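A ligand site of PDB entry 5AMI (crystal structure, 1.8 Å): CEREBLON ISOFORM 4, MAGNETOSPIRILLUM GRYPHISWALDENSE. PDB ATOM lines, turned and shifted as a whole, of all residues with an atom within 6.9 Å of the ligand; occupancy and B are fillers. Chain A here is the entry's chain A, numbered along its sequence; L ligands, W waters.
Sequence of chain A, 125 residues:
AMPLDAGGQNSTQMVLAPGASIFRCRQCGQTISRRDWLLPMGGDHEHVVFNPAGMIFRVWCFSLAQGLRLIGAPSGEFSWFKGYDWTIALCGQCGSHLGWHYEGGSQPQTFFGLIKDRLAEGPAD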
ATOM      1  N   VAL A  49       0.788  19.783 -15.677  1.00  0.00           N
ATOM      2  CA  VAL A  49       0.802  18.796 -14.574  1.00  0.00           C
ATOM      3  C   VAL A  49       1.478  19.381 -13.310  1.00  0.00           C
ATOM      4  O   VAL A  49       2.251  20.323 -13.404  1.00  0.00           O
ATOM      5  CB  VAL A  49       1.515  17.506 -14.982  1.00  0.00           C
ATOM      6  CG1 VAL A  49       0.633  16.830 -16.037  1.00  0.00           C
ATOM      7  CG2 VAL A  49       2.906  17.751 -15.451  1.00  0.00           C
ATOM      8  N   PHE A  50       1.148  18.829 -12.151  1.00  0.00           N
ATOM      9  CA  PHE A  50       1.786  19.183 -10.879  1.00  0.00           C
ATOM     10  C   PHE A  50       2.418  17.945 -10.250  1.00  0.00           C
ATOM     11  O   PHE A  50       1.895  16.822 -10.302  1.00  0.00           O
ATOM     12  CB  PHE A  50       0.770  19.649  -9.836  1.00  0.00           C
ATOM     13  CG  PHE A  50       0.134  20.952 -10.130  1.00  0.00           C
ATOM     14  CD1 PHE A  50      -1.053  21.003 -10.864  1.00  0.00           C
ATOM     15  CD2 PHE A  50       0.633  22.146  -9.572  1.00  0.00           C
ATOM     16  CE1 PHE A  50      -1.669  22.225 -11.097  1.00  0.00           C
ATOM     17  CE2 PHE A  50      -0.014  23.373  -9.798  1.00  0.00           C
ATOM     18  CZ  PHE A  50      -1.168  23.399 -10.561  1.00  0.00           C
ATOM     19  N   ASN A  51       3.562  18.142  -9.651  1.00  0.00           N
ATOM     20  CA  ASN A  51       4.159  17.086  -8.851  1.00  0.00           C
ATOM     21  C   ASN A  51       3.735  17.158  -7.374  1.00  0.00           C
ATOM     22  O   ASN A  51       2.973  18.037  -6.943  1.00  0.00           O
ATOM     23  CB  ASN A  51       5.680  17.121  -9.038  1.00  0.00           C
ATOM     24  CG  ASN A  51       6.386  18.286  -8.401  1.00  0.00           C
ATOM     25  OD1 ASN A  51       5.811  19.004  -7.623  1.00  0.00           O
ATOM     26  ND2 ASN A  51       7.682  18.429  -8.699  1.00  0.00           N
ATOM     27  N   PRO A  52       4.211  16.190  -6.565  1.00  0.00           N
ATOM     28  CA  PRO A  52       3.794  16.197  -5.218  1.00  0.00           C
ATOM     29  C   PRO A  52       4.335  17.357  -4.381  1.00  0.00           C
ATOM     30  O   PRO A  52       3.890  17.529  -3.256  1.00  0.00           O
ATOM     31  CB  PRO A  52       4.301  14.859  -4.680  1.00  0.00           C
ATOM     32  CG  PRO A  52       4.465  13.975  -5.898  1.00  0.00           C
ATOM     33  CD  PRO A  52       4.846  14.908  -6.985  1.00  0.00           C
ATOM     34  N   ALA A  53       5.367  18.039  -4.863  1.00  0.00           N
ATOM     35  CA  ALA A  53       5.912  19.244  -4.177  1.00  0.00           C
ATOM     36  C   ALA A  53       5.132  20.483  -4.625  1.00  0.00           C
ATOM     37  O   ALA A  53       5.527  21.612  -4.298  1.00  0.00           O
ATOM     38  CB  ALA A  53       7.373  19.424  -4.514  1.00  0.00           C
ATOM     39  N   MET A  55       4.764  21.794  -7.554  1.00  0.00           N
ATOM     40  CA  MET A  55       5.305  22.521  -8.701  1.00  0.00           C
ATOM     41  C   MET A  55       4.511  22.202  -9.945  1.00  0.00           C
ATOM     42  O   MET A  55       4.202  21.020 -10.150  1.00  0.00           O
ATOM     43  CB  MET A  55       6.758  22.189  -8.920  1.00  0.00           C
ATOM     44  CG  MET A  55       7.600  22.437  -7.718  1.00  0.00           C
ATOM     45  SD  MET A  55       9.297  21.978  -8.011  1.00  0.00           S
ATOM     46  CE  MET A  55       9.433  20.295  -7.622  1.00  0.00           C
ATOM     47  N   PHE A  57       4.233  22.160 -14.100  1.00  0.00           N
ATOM     48  CA  PHE A  57       5.110  22.053 -15.263  1.00  0.00           C
ATOM     49  C   PHE A  57       4.242  22.039 -16.547  1.00  0.00           C
ATOM     50  O   PHE A  57       3.223  21.383 -16.579  1.00  0.00           O
ATOM     51  CB  PHE A  57       5.890  20.758 -15.254  1.00  0.00           C
ATOM     52  CG  PHE A  57       6.786  20.599 -14.055  1.00  0.00           C
ATOM     53  CD1 PHE A  57       8.048  21.173 -14.016  1.00  0.00           C
ATOM     54  CD2 PHE A  57       6.336  19.908 -12.950  1.00  0.00           C
ATOM     55  CE1 PHE A  57       8.859  21.021 -12.896  1.00  0.00           C
ATOM     56  CE2 PHE A  57       7.154  19.734 -11.836  1.00  0.00           C
ATOM     57  CZ  PHE A  57       8.427  20.278 -11.824  1.00  0.00           C
ATOM     58  N   SER A  75      10.855   4.624 -12.291  1.00  0.00           N
ATOM     59  CA  SER A  75       9.878   4.523 -11.281  1.00  0.00           C
ATOM     60  C   SER A  75       8.485   4.769 -11.864  1.00  0.00           C
ATOM     61  O   SER A  75       8.296   5.729 -12.610  1.00  0.00           O
ATOM     62  CB  SER A  75      10.201   5.556 -10.216  1.00  0.00           C
ATOM     63  OG  SER A  75       9.254   5.419  -9.185  1.00  0.00           O
ATOM     64  N   GLY A  76       7.524   3.969 -11.434  1.00  0.00           N
ATOM     65  CA  GLY A  76       6.083   4.202 -11.695  1.00  0.00           C
ATOM     66  C   GLY A  76       5.375   5.203 -10.775  1.00  0.00           C
ATOM     67  O   GLY A  76       4.295   5.680 -11.066  1.00  0.00           O
ATOM     68  N   GLU A  77       6.003   5.550  -9.688  1.00  0.00           N
ATOM     69  CA  GLU A  77       5.321   6.327  -8.629  1.00  0.00           C
ATOM     70  C   GLU A  77       4.976   7.760  -9.111  1.00  0.00           C
ATOM     71  O   GLU A  77       5.828   8.465  -9.650  1.00  0.00           O
ATOM     72  CB  GLU A  77       6.237   6.334  -7.377  1.00  0.00           C
ATOM     73  CG  GLU A  77       6.683   4.886  -7.068  1.00  0.00           C
ATOM     74  CD  GLU A  77       7.726   4.714  -5.971  1.00  0.00           C
ATOM     75  OE1 GLU A  77       8.703   5.485  -5.925  1.00  0.00           O
ATOM     76  OE2 GLU A  77       7.576   3.749  -5.170  1.00  0.00           O
ATOM     77  N   PHE A  78       3.729   8.169  -8.898  1.00  0.00           N
ATOM     78  CA  PHE A  78       3.245   9.508  -9.314  1.00  0.00           C
ATOM     79  C   PHE A  78       3.344   9.773 -10.805  1.00  0.00           C
ATOM     80  O   PHE A  78       3.304  10.927 -11.219  1.00  0.00           O
ATOM     81  CB  PHE A  78       3.945  10.680  -8.562  1.00  0.00           C
ATOM     82  CG  PHE A  78       3.948  10.561  -7.063  1.00  0.00           C
ATOM     83  CD1 PHE A  78       2.782  10.732  -6.341  1.00  0.00           C
ATOM     84  CD2 PHE A  78       5.117  10.328  -6.367  1.00  0.00           C
ATOM     85  CE1 PHE A  78       2.773  10.630  -4.954  1.00  0.00           C
ATOM     86  CE2 PHE A  78       5.118  10.224  -4.978  1.00  0.00           C
ATOM     87  CZ  PHE A  78       3.941  10.356  -4.288  1.00  0.00           C
ATOM     88  N   SER A  79       3.482   8.752 -11.640  1.00  0.00           N
ATOM     89  CA  SER A  79       3.612   8.991 -13.066  1.00  0.00           C
ATOM     90  C   SER A  79       2.379   9.696 -13.615  1.00  0.00           C
ATOM     91  O   SER A  79       1.277   9.321 -13.326  1.00  0.00           O
ATOM     92  CB  SER A  79       3.803   7.686 -13.799  1.00  0.00           C
ATOM     93  OG  SER A  79       4.001   7.960 -15.172  1.00  0.00           O
ATOM     94  N   TRP A  80       2.594  10.761 -14.383  1.00  0.00           N
ATOM     95  CA  TRP A  80       1.495  11.467 -15.008  1.00  0.00           C
ATOM     96  C   TRP A  80       0.966  10.735 -16.225  1.00  0.00           C
ATOM     97  O   TRP A  80      -0.088  11.115 -16.751  1.00  0.00           O
ATOM     98  CB  TRP A  80       1.950  12.843 -15.505  1.00  0.00           C
ATOM     99  CG  TRP A  80       2.363  13.760 -14.342  1.00  0.00           C
ATOM    100  CD1 TRP A  80       1.620  14.121 -13.256  1.00  0.00           C
ATOM    101  CD2 TRP A  80       3.562  14.473 -14.272  1.00  0.00           C
ATOM    102  NE1 TRP A  80       2.325  14.987 -12.481  1.00  0.00           N
ATOM    103  CE2 TRP A  80       3.521  15.233 -13.056  1.00  0.00           C
ATOM    104  CE3 TRP A  80       4.700  14.529 -15.069  1.00  0.00           C
ATOM    105  CZ2 TRP A  80       4.570  16.023 -12.642  1.00  0.00           C
ATOM    106  CZ3 TRP A  80       5.761  15.334 -14.696  1.00  0.00           C
ATOM    107  CH2 TRP A  80       5.681  16.099 -13.445  1.00  0.00           C
ATOM    108  N   PHE A  81       1.634   9.657 -16.653  1.00  0.00           N
ATOM    109  CA  PHE A  81       1.223   8.983 -17.877  1.00  0.00           C
ATOM    110  C   PHE A  81       1.052   7.514 -17.551  1.00  0.00           C
ATOM    111  O   PHE A  81       2.010   6.811 -17.208  1.00  0.00           O
ATOM    112  CB  PHE A  81       2.255   9.179 -18.944  1.00  0.00           C
ATOM    113  CG  PHE A  81       2.478  10.628 -19.330  1.00  0.00           C
ATOM    114  CD1 PHE A  81       1.600  11.255 -20.157  1.00  0.00           C
ATOM    115  CD2 PHE A  81       3.570  11.334 -18.864  1.00  0.00           C
ATOM    116  CE1 PHE A  81       1.769  12.616 -20.478  1.00  0.00           C
ATOM    117  CE2 PHE A  81       3.757  12.721 -19.194  1.00  0.00           C
ATOM    118  CZ  PHE A  81       2.848  13.330 -19.993  1.00  0.00           C
ATOM    119  N   TYR A  84       3.426   4.069 -17.724  1.00  0.00           N
ATOM    120  CA  TYR A  84       4.844   4.422 -17.951  1.00  0.00           C
ATOM    121  C   TYR A  84       5.591   4.631 -16.649  1.00  0.00           C
ATOM    122  O   TYR A  84       5.046   5.238 -15.698  1.00  0.00           O
ATOM    123  CB  TYR A  84       5.038   5.688 -18.851  1.00  0.00           C
ATOM    124  CG  TYR A  84       4.499   5.526 -20.239  1.00  0.00           C
ATOM    125  CD1 TYR A  84       3.169   5.842 -20.544  1.00  0.00           C
ATOM    126  CD2 TYR A  84       5.312   5.061 -21.266  1.00  0.00           C
ATOM    127  CE1 TYR A  84       2.707   5.708 -21.833  1.00  0.00           C
ATOM    128  CE2 TYR A  84       4.865   4.953 -22.551  1.00  0.00           C
ATOM    129  CZ  TYR A  84       3.538   5.253 -22.841  1.00  0.00           C
ATOM    130  OH  TYR A  84       3.051   5.116 -24.114  1.00  0.00           O
ATOM    131  N   TRP A  86       9.138   6.506 -15.095  1.00  0.00           N
ATOM    132  CA  TRP A  86       9.992   7.653 -15.442  1.00  0.00           C
ATOM    133  C   TRP A  86      11.380   7.608 -14.840  1.00  0.00           C
ATOM    134  O   TRP A  86      11.572   7.027 -13.735  1.00  0.00           O
ATOM    135  CB  TRP A  86       9.330   9.004 -15.020  1.00  0.00           C
ATOM    136  CG  TRP A  86       8.888   9.056 -13.620  1.00  0.00           C
ATOM    137  CD1 TRP A  86       7.669   8.704 -13.126  1.00  0.00           C
ATOM    138  CD2 TRP A  86       9.697   9.388 -12.511  1.00  0.00           C
ATOM    139  NE1 TRP A  86       7.655   8.860 -11.800  1.00  0.00           N
ATOM    140  CE2 TRP A  86       8.876   9.254 -11.353  1.00  0.00           C
ATOM    141  CE3 TRP A  86      11.040   9.780 -12.354  1.00  0.00           C
ATOM    142  CZ2 TRP A  86       9.335   9.498 -10.084  1.00  0.00           C
ATOM    143  CZ3 TRP A  86      11.498  10.037 -11.071  1.00  0.00           C
ATOM    144  CH2 TRP A  86      10.640   9.891  -9.944  1.00  0.00           C
ATOM    145  N   THR A  87      12.322   8.271 -15.526  1.00  0.00           N
ATOM    146  CA  THR A  87      13.646   8.535 -15.049  1.00  0.00           C
ATOM    147  C   THR A  87      13.881  10.035 -15.263  1.00  0.00           C
ATOM    148  O   THR A  87      13.406  10.611 -16.241  1.00  0.00           O
ATOM    149  CB  THR A  87      14.710   7.743 -15.789  1.00  0.00           C
ATOM    150  OG1 THR A  87      14.602   8.074 -17.148  1.00  0.00           O
ATOM    151  CG2 THR A  87      14.458   6.253 -15.667  1.00  0.00           C
ATOM    152  N   ILE A  88      14.526  10.655 -14.319  1.00  0.00           N
ATOM    153  CA  ILE A  88      14.905  12.059 -14.478  1.00  0.00           C
ATOM    154  C   ILE A  88      15.833  12.296 -15.643  1.00  0.00           C
ATOM    155  O   ILE A  88      16.841  11.567 -15.791  1.00  0.00           O
ATOM    156  CB  ILE A  88      15.578  12.556 -13.187  1.00  0.00           C
ATOM    157  CG1 ILE A  88      14.481  12.580 -12.094  1.00  0.00           C
ATOM    158  CG2 ILE A  88      16.207  13.921 -13.366  1.00  0.00           C
ATOM    159  CD1 ILE A  88      15.065  12.618 -10.697  1.00  0.00           C
ATOM    160  N   HIS A  97      17.841  20.298 -14.917  1.00  0.00           N
ATOM    161  CA  HIS A  97      16.758  19.342 -15.030  1.00  0.00           C
ATOM    162  C   HIS A  97      15.754  19.739 -16.141  1.00  0.00           C
ATOM    163  O   HIS A  97      15.104  20.734 -16.030  1.00  0.00           O
ATOM    164  CB  HIS A  97      16.078  19.190 -13.685  1.00  0.00           C
ATOM    165  CG  HIS A  97      14.930  18.279 -13.748  1.00  0.00           C
ATOM    166  ND1 HIS A  97      13.848  18.420 -12.925  1.00  0.00           N
ATOM    167  CD2 HIS A  97      14.702  17.192 -14.513  1.00  0.00           C
ATOM    168  CE1 HIS A  97      12.988  17.430 -13.158  1.00  0.00           C
ATOM    169  NE2 HIS A  97      13.461  16.695 -14.144  1.00  0.00           N
ATOM    170  N   TRP A 100      11.792  14.376 -18.080  1.00  0.00           N
ATOM    171  CA  TRP A 100      11.773  12.970 -17.724  1.00  0.00           C
ATOM    172  C   TRP A 100      11.744  12.104 -18.996  1.00  0.00           C
ATOM    173  O   TRP A 100      11.182  12.498 -20.028  1.00  0.00           O
ATOM    174  CB  TRP A 100      10.579  12.630 -16.845  1.00  0.00           C
ATOM    175  CG  TRP A 100      10.503  13.447 -15.614  1.00  0.00           C
ATOM    176  CD1 TRP A 100      10.994  13.105 -14.416  1.00  0.00           C
ATOM    177  CD2 TRP A 100       9.926  14.743 -15.464  1.00  0.00           C
ATOM    178  NE1 TRP A 100      10.793  14.098 -13.518  1.00  0.00           N
ATOM    179  CE2 TRP A 100      10.166  15.131 -14.122  1.00  0.00           C
ATOM    180  CE3 TRP A 100       9.239  15.603 -16.319  1.00  0.00           C
ATOM    181  CZ2 TRP A 100       9.700  16.344 -13.590  1.00  0.00           C
ATOM    182  CZ3 TRP A 100       8.849  16.846 -15.812  1.00  0.00           C
ATOM    183  CH2 TRP A 100       9.036  17.187 -14.469  1.00  0.00           C
ATOM    184  N   TYR A 102      10.254   8.451 -20.290  1.00  0.00           N
ATOM    185  CA  TYR A 102       9.226   7.516 -19.915  1.00  0.00           C
ATOM    186  C   TYR A 102       9.457   6.240 -20.659  1.00  0.00           C
ATOM    187  O   TYR A 102       9.816   6.297 -21.837  1.00  0.00           O
ATOM    188  CB  TYR A 102       7.826   8.098 -20.223  1.00  0.00           C
ATOM    189  CG  TYR A 102       7.471   9.210 -19.280  1.00  0.00           C
ATOM    190  CD1 TYR A 102       6.925   8.911 -18.052  1.00  0.00           C
ATOM    191  CD2 TYR A 102       7.752  10.550 -19.603  1.00  0.00           C
ATOM    192  CE1 TYR A 102       6.564   9.972 -17.170  1.00  0.00           C
ATOM    193  CE2 TYR A 102       7.455  11.583 -18.706  1.00  0.00           C
ATOM    194  CZ  TYR A 102       6.828  11.252 -17.520  1.00  0.00           C
ATOM    195  OH  TYR A 102       6.584  12.312 -16.645  1.00  0.00           O
HETATM  196  O1  LIG L   1       5.208  13.785 -10.191  1.00  0.00           O
HETATM  197  C1  LIG L   1       5.950  13.446 -11.080  1.00  0.00           C
HETATM  198  N1  LIG L   1       5.349  12.599 -12.099  1.00  0.00           N
HETATM  199  C2  LIG L   1       6.084  12.165 -13.254  1.00  0.00           C
HETATM  200  O2  LIG L   1       5.465  11.556 -14.126  1.00  0.00           O
HETATM  201  C3  LIG L   1       7.555  12.522 -13.264  1.00  0.00           C
HETATM  202  C4  LIG L   1       8.180  12.576 -11.893  1.00  0.00           C
HETATM  203  C5  LIG L   1       7.459  13.728 -11.140  1.00  0.00           C
HETATM  204  N2  LIG L   1       7.924  13.865  -9.814  1.00  0.00           N
HETATM  205  C6  LIG L   1       9.247  15.323  -5.524  1.00  0.00           C
HETATM  206  C7  LIG L   1       9.193  15.800  -6.851  1.00  0.00           C
HETATM  207  C8  LIG L   1       8.729  14.916  -7.816  1.00  0.00           C
HETATM  208  C9  LIG L   1       8.300  13.669  -7.491  1.00  0.00           C
HETATM  209  O3  LIG L   1       8.665  16.037 -10.078  1.00  0.00           O
HETATM  210  O4  LIG L   1       7.257  11.751  -8.810  1.00  0.00           O
HETATM  211  C10 LIG L   1       8.284  13.192  -6.180  1.00  0.00           C
HETATM  212  C11 LIG L   1       8.813  14.049  -5.200  1.00  0.00           C
HETATM  213  C12 LIG L   1       7.699  13.049  -8.664  1.00  0.00           C
HETATM  214  C13 LIG L   1       8.393  15.099  -9.227  1.00  0.00           C
HETATM  215  O   HOH W   1      11.549  14.176 -10.665  1.00  0.00           O
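The backbone NH of Trp 86 is in hydrogen-bond range of the backbone carbonyl oxygen of Ser 75, at 2.7 Å. NE1 of Trp 86 is in hydrogen-bond range of O of Glu 77 (2.8 Å). N of Glu 77 lies within hydrogen-bond range of OG of Ser 75 (3.3 Å). N of Ala 53 lies within hydrogen-bond range of OD1 of Asn 51 (3.0 Å). N of Met 55 sits at hydrogen-bond distance from OD1 of Asn 51 (3.0 Å). OG of Ser 79 lies within hydrogen-bond range of O of Phe 81. NE1 of Trp 80 is in hydrogen-bond range of O of Phe 50 (2.9 Å). The backbone carbonyl oxygen (O) of Tyr 84 is in hydrogen-bond range of the side-chain hydroxyl (OG) of Ser 79, 3.0 Å away.
Residues that only touch the ligand: Pro 52, Glu 77, Ser 79, Trp 86 and Trp 100. Hydrophobic or aromatic side chains that line the ligand: Pro 52, Phe 78, Trp 80, Trp 86, Trp 100 and Tyr 102. Within 4 Å of the ligand: Asn 51, Pro 52, Glu 77, Phe 78, Ser 79, Trp 80, Trp 86, Trp 100 and Tyr 102.
An oxygen (O2) of the ligand sits at hydrogen-bond distance from the backbone NH (N) of Trp 80, 3.0 Å away. A nitrogen (N1) of the ligand lies within hydrogen-bond range of the backbone carbonyl oxygen (O) of Phe 78 (2.8 Å). ND2 of Asn 51 lies within hydrogen-bond range of O3 of the ligand, at 2.9 Å. OH of Tyr 102 is in hydrogen-bond range of O2 of the ligand.
Water W1 lies within hydrogen-bond range of NE1 of Trp 100 (3.0 Å) and O3 of the ligand (3.5 Å).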
